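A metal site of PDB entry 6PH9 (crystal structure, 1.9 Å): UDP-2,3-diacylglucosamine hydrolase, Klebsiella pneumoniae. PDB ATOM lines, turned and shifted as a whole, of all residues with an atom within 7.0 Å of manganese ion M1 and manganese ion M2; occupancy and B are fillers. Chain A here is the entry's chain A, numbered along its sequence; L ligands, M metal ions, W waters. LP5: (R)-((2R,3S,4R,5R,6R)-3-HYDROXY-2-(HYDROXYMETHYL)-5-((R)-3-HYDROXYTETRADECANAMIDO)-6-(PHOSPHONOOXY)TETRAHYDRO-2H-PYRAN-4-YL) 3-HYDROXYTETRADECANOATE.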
ATOM      1  N   ALA A   8       8.778  14.067 -18.415  1.00  0.00           N
ATOM      2  CA  ALA A   8       8.339  15.452 -18.378  1.00  0.00           C
ATOM      3  C   ALA A   8       8.859  16.101 -17.110  1.00  0.00           C
ATOM      4  O   ALA A   8       9.289  15.414 -16.175  1.00  0.00           O
ATOM      5  CB  ALA A   8       6.810  15.564 -18.444  1.00  0.00           C
ATOM      6  N   ASP A   9       8.793  17.432 -17.079  1.00  0.00           N
ATOM      7  CA  ASP A   9       9.060  18.220 -15.879  1.00  0.00           C
ATOM      8  C   ASP A   9      10.455  17.970 -15.320  1.00  0.00           C
ATOM      9  O   ASP A   9      10.647  17.812 -14.106  1.00  0.00           O
ATOM     10  CB  ASP A   9       7.984  17.967 -14.817  1.00  0.00           C
ATOM     11  CG  ASP A   9       6.601  18.367 -15.300  1.00  0.00           C
ATOM     12  OD1 ASP A   9       6.367  19.569 -15.499  1.00  0.00           O
ATOM     13  OD2 ASP A   9       5.758  17.458 -15.509  1.00  0.00           O
ATOM     14  N   LEU A  10      11.454  17.927 -16.209  1.00  0.00           N
ATOM     15  CA  LEU A  10      12.836  17.851 -15.765  1.00  0.00           C
ATOM     16  C   LEU A  10      13.327  19.190 -15.236  1.00  0.00           C
ATOM     17  O   LEU A  10      14.165  19.226 -14.333  1.00  0.00           O
ATOM     18  CB  LEU A  10      13.719  17.361 -16.915  1.00  0.00           C
ATOM     19  CG  LEU A  10      13.519  15.910 -17.355  1.00  0.00           C
ATOM     20  CD1 LEU A  10      12.431  15.797 -18.429  1.00  0.00           C
ATOM     21  CD2 LEU A  10      14.825  15.336 -17.855  1.00  0.00           C
ATOM     22  N   HIS A  11      12.803  20.292 -15.785  1.00  0.00           N
ATOM     23  CA  HIS A  11      13.146  21.647 -15.353  1.00  0.00           C
ATOM     24  C   HIS A  11      14.654  21.844 -15.297  1.00  0.00           C
ATOM     25  O   HIS A  11      15.218  22.352 -14.323  1.00  0.00           O
ATOM     26  CB  HIS A  11      12.497  21.955 -14.003  1.00  0.00           C
ATOM     27  CG  HIS A  11      11.004  22.113 -14.057  1.00  0.00           C
ATOM     28  ND1 HIS A  11      10.397  23.343 -14.212  1.00  0.00           N
ATOM     29  CD2 HIS A  11      10.008  21.201 -13.975  1.00  0.00           C
ATOM     30  CE1 HIS A  11       9.085  23.179 -14.224  1.00  0.00           C
ATOM     31  NE2 HIS A  11       8.821  21.892 -14.088  1.00  0.00           N
ATOM     32  N   LEU A  40       7.085  15.370 -22.556  1.00  0.00           N
ATOM     33  CA  LEU A  40       5.792  16.052 -22.445  1.00  0.00           C
ATOM     34  C   LEU A  40       5.884  17.406 -21.758  1.00  0.00           C
ATOM     35  O   LEU A  40       5.042  17.733 -20.915  1.00  0.00           O
ATOM     36  CB  LEU A  40       4.796  15.147 -21.730  1.00  0.00           C
ATOM     37  CG  LEU A  40       4.573  13.771 -22.358  1.00  0.00           C
ATOM     38  CD1 LEU A  40       3.411  13.052 -21.689  1.00  0.00           C
ATOM     39  CD2 LEU A  40       4.328  13.896 -23.858  1.00  0.00           C
ATOM     40  N   GLY A  41       6.884  18.220 -22.085  1.00  0.00           N
ATOM     41  CA  GLY A  41       6.891  19.595 -21.626  1.00  0.00           C
ATOM     42  C   GLY A  41       7.735  19.799 -20.378  1.00  0.00           C
ATOM     43  O   GLY A  41       7.996  18.879 -19.597  1.00  0.00           O
ATOM     44  N   ASP A  42       8.125  21.060 -20.175  1.00  0.00           N
ATOM     45  CA  ASP A  42       8.967  21.455 -19.049  1.00  0.00           C
ATOM     46  C   ASP A  42      10.257  20.656 -19.017  1.00  0.00           C
ATOM     47  O   ASP A  42      10.716  20.201 -17.965  1.00  0.00           O
ATOM     48  CB  ASP A  42       8.215  21.339 -17.720  1.00  0.00           C
ATOM     49  CG  ASP A  42       7.124  22.388 -17.583  1.00  0.00           C
ATOM     50  OD1 ASP A  42       7.012  23.250 -18.470  1.00  0.00           O
ATOM     51  OD2 ASP A  42       6.395  22.345 -16.575  1.00  0.00           O
ATOM     52  N   GLY A  79       5.702  22.687 -22.658  1.00  0.00           N
ATOM     53  CA  GLY A  79       5.189  22.937 -21.336  1.00  0.00           C
ATOM     54  C   GLY A  79       4.981  24.427 -21.097  1.00  0.00           C
ATOM     55  O   GLY A  79       5.216  25.262 -21.966  1.00  0.00           O
ATOM     56  N   ASN A  80       4.539  24.745 -19.885  1.00  0.00           N
ATOM     57  CA  ASN A  80       4.347  26.145 -19.506  1.00  0.00           C
ATOM     58  C   ASN A  80       5.676  26.858 -19.301  1.00  0.00           C
ATOM     59  O   ASN A  80       5.697  28.100 -19.297  1.00  0.00           O
ATOM     60  CB  ASN A  80       3.486  26.244 -18.258  1.00  0.00           C
ATOM     61  CG  ASN A  80       4.112  25.572 -17.056  1.00  0.00           C
ATOM     62  OD1 ASN A  80       4.150  24.339 -16.979  1.00  0.00           O
ATOM     63  ND2 ASN A  80       4.603  26.365 -16.113  1.00  0.00           N
ATOM     64  N   ARG A  81       6.763  26.119 -19.132  1.00  0.00           N
ATOM     65  CA  ARG A  81       8.085  26.727 -18.965  1.00  0.00           C
ATOM     66  C   ARG A  81       8.821  26.929 -20.277  1.00  0.00           C
ATOM     67  O   ARG A  81       9.621  27.861 -20.387  1.00  0.00           O
ATOM     68  CB  ARG A  81       8.949  25.872 -18.039  1.00  0.00           C
ATOM     69  CG  ARG A  81       8.405  25.709 -16.627  1.00  0.00           C
ATOM     70  CD  ARG A  81       8.340  27.044 -15.897  1.00  0.00           C
ATOM     71  NE  ARG A  81       7.971  26.850 -14.492  1.00  0.00           N
ATOM     72  CZ  ARG A  81       8.830  26.509 -13.542  1.00  0.00           C
ATOM     73  NH1 ARG A  81      10.105  26.330 -13.841  1.00  0.00           N
ATOM     74  NH2 ARG A  81       8.415  26.348 -12.293  1.00  0.00           N
ATOM     75  N   HIS A 115       0.885  18.145 -21.992  1.00  0.00           N
ATOM     76  CA  HIS A 115       1.649  18.569 -20.825  1.00  0.00           C
ATOM     77  C   HIS A 115       0.808  18.492 -19.562  1.00  0.00           C
ATOM     78  O   HIS A 115       1.282  18.044 -18.510  1.00  0.00           O
ATOM     79  CB  HIS A 115       2.188  19.977 -21.008  1.00  0.00           C
ATOM     80  CG  HIS A 115       2.982  20.458 -19.824  1.00  0.00           C
ATOM     81  ND1 HIS A 115       4.113  19.812 -19.385  1.00  0.00           N
ATOM     82  CD2 HIS A 115       2.779  21.492 -18.974  1.00  0.00           C
ATOM     83  CE1 HIS A 115       4.588  20.437 -18.316  1.00  0.00           C
ATOM     84  NE2 HIS A 115       3.791  21.459 -18.052  1.00  0.00           N
ATOM     85  N   GLY A 116      -0.460  18.915 -19.641  1.00  0.00           N
ATOM     86  CA  GLY A 116      -1.394  18.806 -18.538  1.00  0.00           C
ATOM     87  C   GLY A 116      -1.900  20.124 -17.997  1.00  0.00           C
ATOM     88  O   GLY A 116      -2.926  20.130 -17.298  1.00  0.00           O
ATOM     89  N   ASP A 117      -1.229  21.233 -18.279  1.00  0.00           N
ATOM     90  CA  ASP A 117      -1.657  22.510 -17.715  1.00  0.00           C
ATOM     91  C   ASP A 117      -3.026  22.933 -18.235  1.00  0.00           C
ATOM     92  O   ASP A 117      -3.780  23.609 -17.520  1.00  0.00           O
ATOM     93  CB  ASP A 117      -0.620  23.605 -18.023  1.00  0.00           C
ATOM     94  CG  ASP A 117      -0.374  23.760 -19.510  1.00  0.00           C
ATOM     95  OD1 ASP A 117       0.029  22.774 -20.160  1.00  0.00           O
ATOM     96  OD2 ASP A 117      -0.580  24.883 -20.026  1.00  0.00           O
ATOM     97  N   TYR A 126      -4.490  31.560 -14.638  1.00  0.00           N
ATOM     98  CA  TYR A 126      -3.444  30.918 -15.432  1.00  0.00           C
ATOM     99  C   TYR A 126      -3.834  30.837 -16.895  1.00  0.00           C
ATOM    100  O   TYR A 126      -3.015  31.153 -17.773  1.00  0.00           O
ATOM    101  CB  TYR A 126      -3.140  29.515 -14.905  1.00  0.00           C
ATOM    102  CG  TYR A 126      -2.275  28.769 -15.904  1.00  0.00           C
ATOM    103  CD1 TYR A 126      -0.974  29.184 -16.137  1.00  0.00           C
ATOM    104  CD2 TYR A 126      -2.788  27.715 -16.653  1.00  0.00           C
ATOM    105  CE1 TYR A 126      -0.183  28.541 -17.067  1.00  0.00           C
ATOM    106  CE2 TYR A 126      -1.990  27.070 -17.590  1.00  0.00           C
ATOM    107  CZ  TYR A 126      -0.691  27.488 -17.795  1.00  0.00           C
ATOM    108  OH  TYR A 126       0.106  26.844 -18.718  1.00  0.00           O
ATOM    109  N   GLY A 195       1.964  15.551 -17.559  1.00  0.00           N
ATOM    110  CA  GLY A 195       2.830  15.978 -16.478  1.00  0.00           C
ATOM    111  C   GLY A 195       2.299  17.214 -15.787  1.00  0.00           C
ATOM    112  O   GLY A 195       1.120  17.262 -15.417  1.00  0.00           O
ATOM    113  N   HIS A 196       3.172  18.219 -15.588  1.00  0.00           N
ATOM    114  CA  HIS A 196       2.853  19.535 -15.050  1.00  0.00           C
ATOM    115  C   HIS A 196       2.597  19.558 -13.535  1.00  0.00           C
ATOM    116  O   HIS A 196       3.138  20.409 -12.831  1.00  0.00           O
ATOM    117  CB  HIS A 196       1.646  20.156 -15.755  1.00  0.00           C
ATOM    118  CG  HIS A 196       1.322  21.537 -15.289  1.00  0.00           C
ATOM    119  ND1 HIS A 196       2.196  22.596 -15.431  1.00  0.00           N
ATOM    120  CD2 HIS A 196       0.238  22.036 -14.652  1.00  0.00           C
ATOM    121  CE1 HIS A 196       1.662  23.682 -14.915  1.00  0.00           C
ATOM    122  NE2 HIS A 196       0.474  23.376 -14.432  1.00  0.00           N
ATOM    123  N   THR A 197       1.761  18.643 -13.036  1.00  0.00           N
ATOM    124  CA  THR A 197       1.335  18.755 -11.635  1.00  0.00           C
ATOM    125  C   THR A 197       2.374  18.214 -10.650  1.00  0.00           C
ATOM    126  O   THR A 197       2.285  18.531  -9.452  1.00  0.00           O
ATOM    127  CB  THR A 197       0.006  18.027 -11.417  1.00  0.00           C
ATOM    128  OG1 THR A 197       0.182  16.617 -11.625  1.00  0.00           O
ATOM    129  CG2 THR A 197      -1.047  18.542 -12.378  1.00  0.00           C
ATOM    130  N   HIS A 198       3.330  17.409 -11.109  1.00  0.00           N
ATOM    131  CA  HIS A 198       4.411  16.876 -10.266  1.00  0.00           C
ATOM    132  C   HIS A 198       3.877  15.953  -9.169  1.00  0.00           C
ATOM    133  O   HIS A 198       4.470  15.844  -8.100  1.00  0.00           O
ATOM    134  CB  HIS A 198       5.253  17.993  -9.639  1.00  0.00           C
ATOM    135  CG  HIS A 198       5.873  18.922 -10.638  1.00  0.00           C
ATOM    136  ND1 HIS A 198       6.793  19.894 -10.282  1.00  0.00           N
ATOM    137  CD2 HIS A 198       5.707  19.040 -11.982  1.00  0.00           C
ATOM    138  CE1 HIS A 198       7.161  20.563 -11.351  1.00  0.00           C
ATOM    139  NE2 HIS A 198       6.520  20.070 -12.403  1.00  0.00           N
ATOM    140  N   ALA A 219       8.148  15.048 -11.444  1.00  0.00           N
ATOM    141  CA  ALA A 219       9.238  15.966 -11.699  1.00  0.00           C
ATOM    142  C   ALA A 219      10.560  15.349 -11.251  1.00  0.00           C
ATOM    143  O   ALA A 219      10.601  14.500 -10.356  1.00  0.00           O
ATOM    144  CB  ALA A 219       9.015  17.296 -10.978  1.00  0.00           C
HETATM  145  O48 LP5 L   1       5.383  26.102 -11.817  1.00  0.00           O
HETATM  146  P45 LP5 L   1       5.041  27.528 -12.193  1.00  0.00           P
HETATM  147  O46 LP5 L   1       5.675  28.474 -11.210  1.00  0.00           O
HETATM  148  O47 LP5 L   1       5.554  27.821 -13.587  1.00  0.00           O
HETATM  149  O1  LP5 L   1       3.402  27.720 -12.160  1.00  0.00           O
HETATM  150  C1  LP5 L   1       2.669  27.419 -13.283  1.00  0.00           C
HETATM  151  C2  LP5 L   1       1.915  28.676 -13.707  1.00  0.00           C
HETATM  152  N2  LP5 L   1       2.890  29.767 -13.961  1.00  0.00           N
HETATM  153  C7  LP5 L   1       3.489  29.880 -15.278  1.00  0.00           C
HETATM  154  C8  LP5 L   1       4.491  30.995 -15.555  1.00  0.00           C
HETATM  155  C16 LP5 L   1       5.833  30.372 -15.890  1.00  0.00           C
HETATM  156  O44 LP5 L   1       6.382  29.768 -14.750  1.00  0.00           O
HETATM  157  C17 LP5 L   1       6.776  31.463 -16.382  1.00  0.00           C
HETATM  158  C18 LP5 L   1       7.927  30.787 -17.136  1.00  0.00           C
HETATM  159  C19 LP5 L   1       8.741  31.856 -17.847  1.00  0.00           C
HETATM  160  C20 LP5 L   1       8.941  31.430 -19.304  1.00  0.00           C
HETATM  161  C21 LP5 L   1      10.054  32.266 -19.911  1.00  0.00           C
HETATM  162  C22 LP5 L   1       9.479  33.632 -20.273  1.00  0.00           C
HETATM  163  C23 LP5 L   1       8.823  33.515 -21.641  1.00  0.00           C
HETATM  164  C24 LP5 L   1       7.770  34.607 -21.800  1.00  0.00           C
HETATM  165  C25 LP5 L   1       7.413  34.724 -23.269  1.00  0.00           C
HETATM  166  C26 LP5 L   1       6.274  35.716 -23.450  1.00  0.00           C
HETATM  167  C27 LP5 L   1       5.865  35.740 -24.920  1.00  0.00           C
HETATM  168  O7  LP5 L   1       3.209  29.102 -16.124  1.00  0.00           O
HETATM  169  C3  LP5 L   1       0.953  29.116 -12.663  1.00  0.00           C
HETATM  170  C4  LP5 L   1       0.047  28.030 -12.256  1.00  0.00           C
HETATM  171  C5  LP5 L   1       0.824  26.777 -11.852  1.00  0.00           C
HETATM  172  O5  LP5 L   1       1.729  26.349 -12.965  1.00  0.00           O
HETATM  173  C6  LP5 L   1      -0.138  25.674 -11.596  1.00  0.00           C
HETATM  174  O6  LP5 L   1      -0.753  25.313 -12.797  1.00  0.00           O
HETATM  175  O4  LP5 L   1      -0.713  28.487 -11.108  1.00  0.00           O
HETATM  176  O3  LP5 L   1       0.139  30.196 -13.212  1.00  0.00           O
HETATM  177  C28 LP5 L   1       0.319  31.436 -12.592  1.00  0.00           C
HETATM  178  O42 LP5 L   1       0.680  31.486 -11.462  1.00  0.00           O
HETATM  179  C29 LP5 L   1       0.044  32.715 -13.374  1.00  0.00           C
HETATM  180  C30 LP5 L   1      -0.796  33.674 -12.533  1.00  0.00           C
HETATM  181  O43 LP5 L   1      -2.045  33.111 -12.259  1.00  0.00           O
HETATM  182  C31 LP5 L   1      -0.958  34.973 -13.332  1.00  0.00           C
HETATM  183  C32 LP5 L   1       0.428  35.583 -13.511  1.00  0.00           C
HETATM  184  C33 LP5 L   1       0.433  36.604 -14.637  1.00  0.00           C
HETATM  185  C34 LP5 L   1       1.193  37.840 -14.172  1.00  0.00           C
HETATM  186  C35 LP5 L   1       2.632  37.774 -14.674  1.00  0.00           C
HETATM  187  C36 LP5 L   1       2.815  38.772 -15.823  1.00  0.00           C
HETATM  188  C37 LP5 L   1       4.222  39.352 -15.783  1.00  0.00           C
HETATM  189  C38 LP5 L   1       4.421  40.237 -17.002  1.00  0.00           C
HETATM  190  C39 LP5 L   1       5.689  41.076 -16.859  1.00  0.00           C
HETATM  191  C40 LP5 L   1       6.002  41.767 -18.184  1.00  0.00           C
HETATM  192  C41 LP5 L   1       7.306  42.546 -18.073  1.00  0.00           C
HETATM  193 MN    MN M   1       6.770  21.045 -14.415  1.00  0.00          MN
HETATM  194 MN    MN M   2       4.317  22.502 -16.245  1.00  0.00          MN
HETATM  195  O   HOH W   1       4.958  22.206 -14.472  1.00  0.00           O
HETATM  196  O   HOH W   2       5.703  24.532 -13.952  1.00  0.00           O
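OD1 of Asp 9 binds manganese ion M1, at 1.9 Å. Water W1 is bound to manganese ion M1 (2.2 Å). Manganese ion M1 is bound by NE2 of His 11 (2.2 Å). A ring nitrogen (NE2) of His 198 binds manganese ion M1 (2.2 Å). The side-chain carboxylate (OD2) of Asp 42 is bound to manganese ion M1, at 2.5 Å.
The side-chain carboxylate of Asp 9 sits at hydrogen-bond distance from the backbone NH of His 196. The backbone carbonyl oxygen (O) of Gly 41 lies within hydrogen-bond range of the backbone NH (N) of Asp 9, 3.0 Å away. The backbone NH (N) of Arg 81 lies within hydrogen-bond range of the side-chain carboxylate (OD1) of Asp 42 (3.0 Å). N of Leu 10 lies within hydrogen-bond range of O of Asp 42, 3.0 Å away. The backbone carbonyl oxygen (O) of His 115 is in hydrogen-bond range of the backbone NH (N) of Gly 195, at 2.8 Å. O of Leu 40 is in hydrogen-bond range of ND1 of His 115 (2.7 Å). A ring nitrogen (ND1) of His 11 lies within hydrogen-bond range of the guanidinium group of Arg 81 (3.0 Å). O of His 196 lies close to NE2 of His 198, 3.4 Å away.
Along chain A the residues within 4 Å of manganese ion M2 span positions 9 to 196.
Four residues have an atom within 4 Å of manganese ion M1: Asp 9, His 11, Asp 42 and His 198. The nearest printed residue that does not touch manganese ion M1 is His 196 (4.01 Å).
The side-chain amide nitrogen (ND2) of Asn 80 is in hydrogen-bond range of an oxygen (O47) of the ligand. NE2 of His 196 is in hydrogen-bond range of O6 of the ligand. O47 of the ligand lies within salt-bridge range of NE of Arg 81 (2.8 Å).
Water W2 lies within hydrogen-bond range of an oxygen (O48) of the ligand, the side-chain amide nitrogen (ND2) of Asn 80 and the guanidinium group (NE) of Arg 81.
Manganese ion M2 is bound by water W1 (1.9 Å), the side-chain amide oxygen of Asn 80 (2.0 Å), the side-chain carboxylate of Asp 42 (2.1 Å), a ring nitrogen (NE2) of His 115 (2.2 Å) and a ring nitrogen (ND1) of His 196 (2.3 Å). Manganese ion M2 has five donor atoms within binding distance.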
